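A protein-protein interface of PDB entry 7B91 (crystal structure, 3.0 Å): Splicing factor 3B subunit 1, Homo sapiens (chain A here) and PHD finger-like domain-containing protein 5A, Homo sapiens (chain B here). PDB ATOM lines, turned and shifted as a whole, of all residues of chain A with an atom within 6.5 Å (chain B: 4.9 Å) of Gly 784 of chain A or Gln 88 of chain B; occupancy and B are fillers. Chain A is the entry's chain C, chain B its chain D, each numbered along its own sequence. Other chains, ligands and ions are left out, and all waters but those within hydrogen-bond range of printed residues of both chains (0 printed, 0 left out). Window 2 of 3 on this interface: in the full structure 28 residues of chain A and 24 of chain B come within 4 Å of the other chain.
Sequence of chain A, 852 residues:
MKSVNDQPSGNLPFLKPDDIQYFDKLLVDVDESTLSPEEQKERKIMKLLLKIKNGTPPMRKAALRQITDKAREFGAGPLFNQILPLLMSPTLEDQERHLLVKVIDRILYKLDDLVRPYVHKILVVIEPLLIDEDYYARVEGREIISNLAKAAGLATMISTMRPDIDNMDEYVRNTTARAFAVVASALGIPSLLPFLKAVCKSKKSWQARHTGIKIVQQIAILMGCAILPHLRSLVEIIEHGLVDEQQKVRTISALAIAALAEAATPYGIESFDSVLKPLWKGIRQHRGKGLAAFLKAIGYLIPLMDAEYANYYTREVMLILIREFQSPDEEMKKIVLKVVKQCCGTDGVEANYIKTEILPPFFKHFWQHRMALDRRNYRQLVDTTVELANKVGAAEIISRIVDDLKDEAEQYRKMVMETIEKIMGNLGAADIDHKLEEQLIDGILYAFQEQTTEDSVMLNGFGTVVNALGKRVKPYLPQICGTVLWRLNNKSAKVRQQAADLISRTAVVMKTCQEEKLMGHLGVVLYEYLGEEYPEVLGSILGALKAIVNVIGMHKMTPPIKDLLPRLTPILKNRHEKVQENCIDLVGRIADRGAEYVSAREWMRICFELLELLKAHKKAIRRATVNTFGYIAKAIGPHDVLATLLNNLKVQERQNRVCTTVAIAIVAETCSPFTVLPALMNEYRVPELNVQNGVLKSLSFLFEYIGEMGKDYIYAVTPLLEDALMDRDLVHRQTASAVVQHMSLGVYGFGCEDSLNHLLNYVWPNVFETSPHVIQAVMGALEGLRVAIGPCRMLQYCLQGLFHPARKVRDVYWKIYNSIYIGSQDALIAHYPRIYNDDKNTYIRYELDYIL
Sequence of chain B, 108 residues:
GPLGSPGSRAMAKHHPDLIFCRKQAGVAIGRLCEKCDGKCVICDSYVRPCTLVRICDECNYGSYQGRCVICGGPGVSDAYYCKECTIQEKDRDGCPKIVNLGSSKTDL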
ATOM      1  N   VAL A 740     -10.627 -31.938  -1.159  1.00  0.00           N
ATOM      2  CA  VAL A 740     -10.053 -30.752  -1.795  1.00  0.00           C
ATOM      3  C   VAL A 740     -10.646 -29.482  -1.200  1.00  0.00           C
ATOM      4  O   VAL A 740      -9.978 -28.440  -1.155  1.00  0.00           O
ATOM      5  CB  VAL A 740     -10.213 -30.790  -3.330  1.00  0.00           C
ATOM      6  CG1 VAL A 740      -9.864 -32.164  -3.874  1.00  0.00           C
ATOM      7  CG2 VAL A 740     -11.606 -30.368  -3.751  1.00  0.00           C
ATOM      8  N   GLN A 741     -11.886 -29.544  -0.706  1.00  0.00           N
ATOM      9  CA  GLN A 741     -12.456 -28.396  -0.011  1.00  0.00           C
ATOM     10  C   GLN A 741     -11.641 -28.053   1.229  1.00  0.00           C
ATOM     11  O   GLN A 741     -11.195 -26.910   1.402  1.00  0.00           O
ATOM     12  CB  GLN A 741     -13.909 -28.678   0.370  1.00  0.00           C
ATOM     13  CG  GLN A 741     -14.449 -27.732   1.428  1.00  0.00           C
ATOM     14  CD  GLN A 741     -15.838 -28.105   1.890  1.00  0.00           C
ATOM     15  OE1 GLN A 741     -16.646 -28.623   1.117  1.00  0.00           O
ATOM     16  NE2 GLN A 741     -16.122 -27.858   3.162  1.00  0.00           N
ATOM     17  N   SER A 744      -8.132 -26.651   0.236  1.00  0.00           N
ATOM     18  CA  SER A 744      -8.068 -25.257  -0.190  1.00  0.00           C
ATOM     19  C   SER A 744      -8.383 -24.306   0.959  1.00  0.00           C
ATOM     20  O   SER A 744      -7.786 -23.228   1.060  1.00  0.00           O
ATOM     21  CB  SER A 744      -9.015 -25.034  -1.368  1.00  0.00           C
ATOM     22  OG  SER A 744     -10.229 -25.729  -1.169  1.00  0.00           O
ATOM     23  N   LEU A 745      -9.301 -24.693   1.851  1.00  0.00           N
ATOM     24  CA  LEU A 745      -9.600 -23.823   2.985  1.00  0.00           C
ATOM     25  C   LEU A 745      -8.453 -23.786   3.990  1.00  0.00           C
ATOM     26  O   LEU A 745      -8.291 -22.788   4.702  1.00  0.00           O
ATOM     27  CB  LEU A 745     -10.898 -24.264   3.664  1.00  0.00           C
ATOM     28  CG  LEU A 745     -12.167 -23.928   2.871  1.00  0.00           C
ATOM     29  CD1 LEU A 745     -13.429 -24.268   3.655  1.00  0.00           C
ATOM     30  CD2 LEU A 745     -12.168 -22.462   2.453  1.00  0.00           C
ATOM     31  N   LEU A 756      -3.901 -26.374  -6.547  1.00  0.00           N
ATOM     32  CA  LEU A 756      -5.349 -26.353  -6.371  1.00  0.00           C
ATOM     33  C   LEU A 756      -6.068 -26.054  -7.681  1.00  0.00           C
ATOM     34  O   LEU A 756      -7.155 -26.590  -7.922  1.00  0.00           O
ATOM     35  CB  LEU A 756      -5.735 -25.339  -5.296  1.00  0.00           C
ATOM     36  CG  LEU A 756      -5.239 -25.643  -3.882  1.00  0.00           C
ATOM     37  CD1 LEU A 756      -5.624 -24.527  -2.927  1.00  0.00           C
ATOM     38  CD2 LEU A 756      -5.779 -26.977  -3.393  1.00  0.00           C
ATOM     39  N   MET A 779     -20.170 -28.570  -4.561  1.00  0.00           N
ATOM     40  CA  MET A 779     -20.355 -27.136  -4.359  1.00  0.00           C
ATOM     41  C   MET A 779     -19.458 -26.612  -3.243  1.00  0.00           C
ATOM     42  O   MET A 779     -18.869 -25.531  -3.371  1.00  0.00           O
ATOM     43  CB  MET A 779     -21.823 -26.831  -4.065  1.00  0.00           C
ATOM     44  CG  MET A 779     -22.721 -26.955  -5.279  1.00  0.00           C
ATOM     45  SD  MET A 779     -22.268 -25.800  -6.586  1.00  0.00           S
ATOM     46  CE  MET A 779     -22.801 -26.716  -8.029  1.00  0.00           C
ATOM     47  N   GLY A 780     -19.343 -27.358  -2.141  1.00  0.00           N
ATOM     48  CA  GLY A 780     -18.434 -26.945  -1.083  1.00  0.00           C
ATOM     49  C   GLY A 780     -16.990 -26.901  -1.548  1.00  0.00           C
ATOM     50  O   GLY A 780     -16.231 -25.994  -1.182  1.00  0.00           O
ATOM     51  N   ALA A 781     -16.594 -27.881  -2.365  1.00  0.00           N
ATOM     52  CA  ALA A 781     -15.255 -27.873  -2.942  1.00  0.00           C
ATOM     53  C   ALA A 781     -15.039 -26.646  -3.820  1.00  0.00           C
ATOM     54  O   ALA A 781     -13.978 -26.015  -3.768  1.00  0.00           O
ATOM     55  CB  ALA A 781     -15.025 -29.152  -3.746  1.00  0.00           C
ATOM     56  N   LEU A 782     -16.038 -26.290  -4.631  1.00  0.00           N
ATOM     57  CA  LEU A 782     -15.898 -25.114  -5.484  1.00  0.00           C
ATOM     58  C   LEU A 782     -15.834 -23.831  -4.666  1.00  0.00           C
ATOM     59  O   LEU A 782     -15.119 -22.897  -5.039  1.00  0.00           O
ATOM     60  CB  LEU A 782     -17.043 -25.046  -6.495  1.00  0.00           C
ATOM     61  CG  LEU A 782     -17.131 -26.197  -7.498  1.00  0.00           C
ATOM     62  CD1 LEU A 782     -18.106 -25.860  -8.615  1.00  0.00           C
ATOM     63  CD2 LEU A 782     -15.759 -26.540  -8.061  1.00  0.00           C
ATOM     64  N   GLU A 783     -16.549 -23.768  -3.542  1.00  0.00           N
ATOM     65  CA  GLU A 783     -16.480 -22.565  -2.716  1.00  0.00           C
ATOM     66  C   GLU A 783     -15.116 -22.436  -2.042  1.00  0.00           C
ATOM     67  O   GLU A 783     -14.519 -21.349  -2.029  1.00  0.00           O
ATOM     68  CB  GLU A 783     -17.604 -22.569  -1.680  1.00  0.00           C
ATOM     69  CG  GLU A 783     -17.964 -21.184  -1.158  1.00  0.00           C
ATOM     70  CD  GLU A 783     -19.200 -21.192  -0.279  1.00  0.00           C
ATOM     71  OE1 GLU A 783     -19.795 -22.277  -0.097  1.00  0.00           O
ATOM     72  OE2 GLU A 783     -19.574 -20.116   0.234  1.00  0.00           O
ATOM     73  N   GLY A 784     -14.604 -23.534  -1.482  1.00  0.00           N
ATOM     74  CA  GLY A 784     -13.257 -23.504  -0.931  1.00  0.00           C
ATOM     75  C   GLY A 784     -12.212 -23.151  -1.975  1.00  0.00           C
ATOM     76  O   GLY A 784     -11.264 -22.406  -1.698  1.00  0.00           O
ATOM     77  N   LEU A 785     -12.376 -23.671  -3.194  1.00  0.00           N
ATOM     78  CA  LEU A 785     -11.451 -23.336  -4.266  1.00  0.00           C
ATOM     79  C   LEU A 785     -11.585 -21.881  -4.692  1.00  0.00           C
ATOM     80  O   LEU A 785     -10.604 -21.281  -5.132  1.00  0.00           O
ATOM     81  CB  LEU A 785     -11.666 -24.267  -5.457  1.00  0.00           C
ATOM     82  CG  LEU A 785     -11.107 -25.673  -5.250  1.00  0.00           C
ATOM     83  CD1 LEU A 785     -11.453 -26.562  -6.430  1.00  0.00           C
ATOM     84  CD2 LEU A 785      -9.601 -25.613  -5.023  1.00  0.00           C
ATOM     85  N   ARG A 786     -12.779 -21.295  -4.582  1.00  0.00           N
ATOM     86  CA  ARG A 786     -12.889 -19.856  -4.797  1.00  0.00           C
ATOM     87  C   ARG A 786     -12.097 -19.098  -3.744  1.00  0.00           C
ATOM     88  O   ARG A 786     -11.367 -18.152  -4.063  1.00  0.00           O
ATOM     89  CB  ARG A 786     -14.348 -19.407  -4.772  1.00  0.00           C
ATOM     90  CG  ARG A 786     -14.494 -17.885  -4.704  1.00  0.00           C
ATOM     91  CD  ARG A 786     -15.944 -17.443  -4.623  1.00  0.00           C
ATOM     92  NE  ARG A 786     -16.606 -17.916  -3.409  1.00  0.00           N
ATOM     93  CZ  ARG A 786     -16.477 -17.341  -2.216  1.00  0.00           C
ATOM     94  NH1 ARG A 786     -15.704 -16.273  -2.074  1.00  0.00           N
ATOM     95  NH2 ARG A 786     -17.118 -17.837  -1.165  1.00  0.00           N
ATOM     96  N   VAL A 787     -12.224 -19.511  -2.483  1.00  0.00           N
ATOM     97  CA  VAL A 787     -11.517 -18.821  -1.406  1.00  0.00           C
ATOM     98  C   VAL A 787     -10.008 -18.882  -1.620  1.00  0.00           C
ATOM     99  O   VAL A 787      -9.305 -17.876  -1.463  1.00  0.00           O
ATOM    100  CB  VAL A 787     -11.917 -19.400  -0.037  1.00  0.00           C
ATOM    101  CG1 VAL A 787     -11.083 -18.765   1.057  1.00  0.00           C
ATOM    102  CG2 VAL A 787     -13.396 -19.159   0.229  1.00  0.00           C
ATOM    103  N   ALA A 788      -9.488 -20.055  -1.990  1.00  0.00           N
ATOM    104  CA  ALA A 788      -8.040 -20.239  -2.096  1.00  0.00           C
ATOM    105  C   ALA A 788      -7.457 -19.760  -3.424  1.00  0.00           C
ATOM    106  O   ALA A 788      -6.368 -19.176  -3.444  1.00  0.00           O
ATOM    107  CB  ALA A 788      -7.679 -21.710  -1.889  1.00  0.00           C
ATOM    108  N   ILE A 789      -8.153 -20.005  -4.536  1.00  0.00           N
ATOM    109  CA  ILE A 789      -7.661 -19.623  -5.856  1.00  0.00           C
ATOM    110  C   ILE A 789      -7.996 -18.171  -6.160  1.00  0.00           C
ATOM    111  O   ILE A 789      -7.194 -17.450  -6.764  1.00  0.00           O
ATOM    112  CB  ILE A 789      -8.253 -20.558  -6.928  1.00  0.00           C
ATOM    113  CG1 ILE A 789      -7.883 -22.012  -6.647  1.00  0.00           C
ATOM    114  CG2 ILE A 789      -7.806 -20.127  -8.321  1.00  0.00           C
ATOM    115  CD1 ILE A 789      -6.504 -22.367  -7.097  1.00  0.00           C
ATOM    116  N   GLY A 823     -20.469 -14.735  -2.561  1.00  0.00           N
ATOM    117  CA  GLY A 823     -19.208 -14.814  -1.837  1.00  0.00           C
ATOM    118  C   GLY A 823     -18.325 -13.594  -2.032  1.00  0.00           C
ATOM    119  O   GLY A 823     -17.781 -13.049  -1.067  1.00  0.00           O
ATOM    120  N   GLU B  84     -13.580 -22.547   9.264  1.00  0.00           N
ATOM    121  CA  GLU B  84     -13.871 -22.702   7.843  1.00  0.00           C
ATOM    122  C   GLU B  84     -15.056 -21.837   7.434  1.00  0.00           C
ATOM    123  O   GLU B  84     -15.041 -21.213   6.367  1.00  0.00           O
ATOM    124  CB  GLU B  84     -14.138 -24.169   7.512  1.00  0.00           C
ATOM    125  CG  GLU B  84     -12.900 -24.954   7.108  1.00  0.00           C
ATOM    126  CD  GLU B  84     -13.243 -26.327   6.563  1.00  0.00           C
ATOM    127  OE1 GLU B  84     -14.410 -26.750   6.708  1.00  0.00           O
ATOM    128  OE2 GLU B  84     -12.347 -26.985   5.994  1.00  0.00           O
ATOM    129  N   CYS B  85     -16.087 -21.781   8.280  1.00  0.00           N
ATOM    130  CA  CYS B  85     -17.223 -20.906   8.006  1.00  0.00           C
ATOM    131  C   CYS B  85     -16.822 -19.438   8.100  1.00  0.00           C
ATOM    132  O   CYS B  85     -17.219 -18.627   7.255  1.00  0.00           O
ATOM    133  CB  CYS B  85     -18.367 -21.220   8.972  1.00  0.00           C
ATOM    134  SG  CYS B  85     -18.973 -22.933   8.909  1.00  0.00           S
ATOM    135  N   THR B  86     -16.028 -19.082   9.114  1.00  0.00           N
ATOM    136  CA  THR B  86     -15.556 -17.707   9.248  1.00  0.00           C
ATOM    137  C   THR B  86     -14.811 -17.254   8.000  1.00  0.00           C
ATOM    138  O   THR B  86     -15.026 -16.141   7.507  1.00  0.00           O
ATOM    139  CB  THR B  86     -14.661 -17.579  10.482  1.00  0.00           C
ATOM    140  OG1 THR B  86     -15.466 -17.629  11.667  1.00  0.00           O
ATOM    141  CG2 THR B  86     -13.877 -16.273  10.455  1.00  0.00           C
ATOM    142  N   ILE B  87     -13.936 -18.109   7.470  1.00  0.00           N
ATOM    143  CA  ILE B  87     -13.189 -17.767   6.264  1.00  0.00           C
ATOM    144  C   ILE B  87     -14.142 -17.557   5.097  1.00  0.00           C
ATOM    145  O   ILE B  87     -13.986 -16.616   4.310  1.00  0.00           O
ATOM    146  CB  ILE B  87     -12.147 -18.861   5.962  1.00  0.00           C
ATOM    147  CG1 ILE B  87     -11.064 -18.876   7.044  1.00  0.00           C
ATOM    148  CG2 ILE B  87     -11.523 -18.640   4.596  1.00  0.00           C
ATOM    149  CD1 ILE B  87     -10.075 -20.011   6.910  1.00  0.00           C
ATOM    150  N   GLN B  88     -15.151 -18.415   4.979  1.00  0.00           N
ATOM    151  CA  GLN B  88     -16.156 -18.292   3.932  1.00  0.00           C
ATOM    152  C   GLN B  88     -17.272 -17.323   4.294  1.00  0.00           C
ATOM    153  O   GLN B  88     -18.241 -17.211   3.534  1.00  0.00           O
ATOM    154  CB  GLN B  88     -16.746 -19.667   3.614  1.00  0.00           C
ATOM    155  CG  GLN B  88     -15.713 -20.702   3.206  1.00  0.00           C
ATOM    156  CD  GLN B  88     -16.296 -22.096   3.126  1.00  0.00           C
ATOM    157  OE1 GLN B  88     -16.818 -22.619   4.109  1.00  0.00           O
ATOM    158  NE2 GLN B  88     -16.218 -22.705   1.949  1.00  0.00           N
ATOM    159  N   GLU B  89     -17.156 -16.630   5.430  1.00  0.00           N
ATOM    160  CA  GLU B  89     -18.142 -15.645   5.885  1.00  0.00           C
ATOM    161  C   GLU B  89     -19.546 -16.234   5.985  1.00  0.00           C
ATOM    162  O   GLU B  89     -20.543 -15.529   5.816  1.00  0.00           O
ATOM    163  CB  GLU B  89     -18.138 -14.400   4.993  1.00  0.00           C
ATOM    164  CG  GLU B  89     -16.822 -13.652   5.049  1.00  0.00           C
ATOM    165  CD  GLU B  89     -16.904 -12.258   4.469  1.00  0.00           C
ATOM    166  OE1 GLU B  89     -17.987 -11.871   3.985  1.00  0.00           O
ATOM    167  OE2 GLU B  89     -15.874 -11.551   4.493  1.00  0.00           O
ATOM    168  N   LYS B  90     -19.634 -17.534   6.274  1.00  0.00           N
ATOM    169  CA  LYS B  90     -20.920 -18.151   6.563  1.00  0.00           C
ATOM    170  C   LYS B  90     -21.474 -17.728   7.915  1.00  0.00           C
ATOM    171  O   LYS B  90     -22.604 -18.100   8.247  1.00  0.00           O
ATOM    172  CB  LYS B  90     -20.796 -19.673   6.502  1.00  0.00           C
ATOM    173  CG  LYS B  90     -20.515 -20.225   5.111  1.00  0.00           C
ATOM    174  CD  LYS B  90     -20.457 -21.744   5.140  1.00  0.00           C
ATOM    175  CE  LYS B  90     -20.406 -22.328   3.743  1.00  0.00           C
ATOM    176  NZ  LYS B  90     -20.335 -23.814   3.785  1.00  0.00           N
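The guanidinium group (NH2) of Arg 786 of chain A lies within salt-bridge range of the side-chain carboxylate (OE2) of Glu 783 of chain A (3.6 Å).
The backbone carbonyl oxygen of Glu 84 of chain B lies close to the side-chain amide oxygen of Gln 88 of chain B, 3.2 Å away.
The backbone carbonyl oxygen (O) of Cys 85 of chain B sits at hydrogen-bond distance from the backbone NH (N) of Lys 90 of chain B, at 2.8 Å.
Among the printed residues, merely in contact across the chains: Leu 745 of chain A with Glu 84 of chain B (3.6 Å), Val 787 of chain A with Ile 87 of chain B (3.6 Å), Leu 745 of chain A with Gln 88 of chain B (3.6 Å), Glu 783 of chain A with Gln 88 of chain B (3.9 Å), Gly 784 of chain A with Gln 88 of chain B (3.9 Å), Glu 783 of chain A with Lys 90 of chain B (3.9 Å) and Leu 745 of chain A with Ile 87 of chain B (3.97 Å).
Of the printed residues of chain B, Leu 745 of chain A touches Glu 84, Ile 87 and Gln 88.
Gly 780 of chain A touches none of the printed residues of chain B.
Of the printed residues of chain B, Glu 783 of chain A touches Gln 88 (3.9 Å) and Lys 90 (3.9 Å).
Gly 784 of chain A touches just one residue of chain B: Gln 88 (3.9 Å).
Arg 786 of chain A touches none of the printed residues of chain B.
Printed residues of chain A within 4 Å of Glu 84 of chain B: Leu 745.
Of the printed residues of chain A, Ile 87 of chain B touches Leu 745 and Val 787.
Gln 88 of chain B touches three residues of chain A.
Of the printed residues of chain A, Lys 90 of chain B touches Glu 783 (3.9 Å).
The nearest residue of chain A that does not touch Gln 88 of chain B is Val 787 of chain A (4.1 Å).
Hydrophobic or aromatic side chains of chain A that line the printed part of chain B: Leu 745 and Val 787.
Printed residues of chain B that touch a printed residue of chain A: Glu 84, Ile 87, Gln 88 and Lys 90.
Hydrophobic or aromatic side chains of chain B that line the printed part of chain A: Ile 87.
Among the printed residues, 7 pairs touch across the chains.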
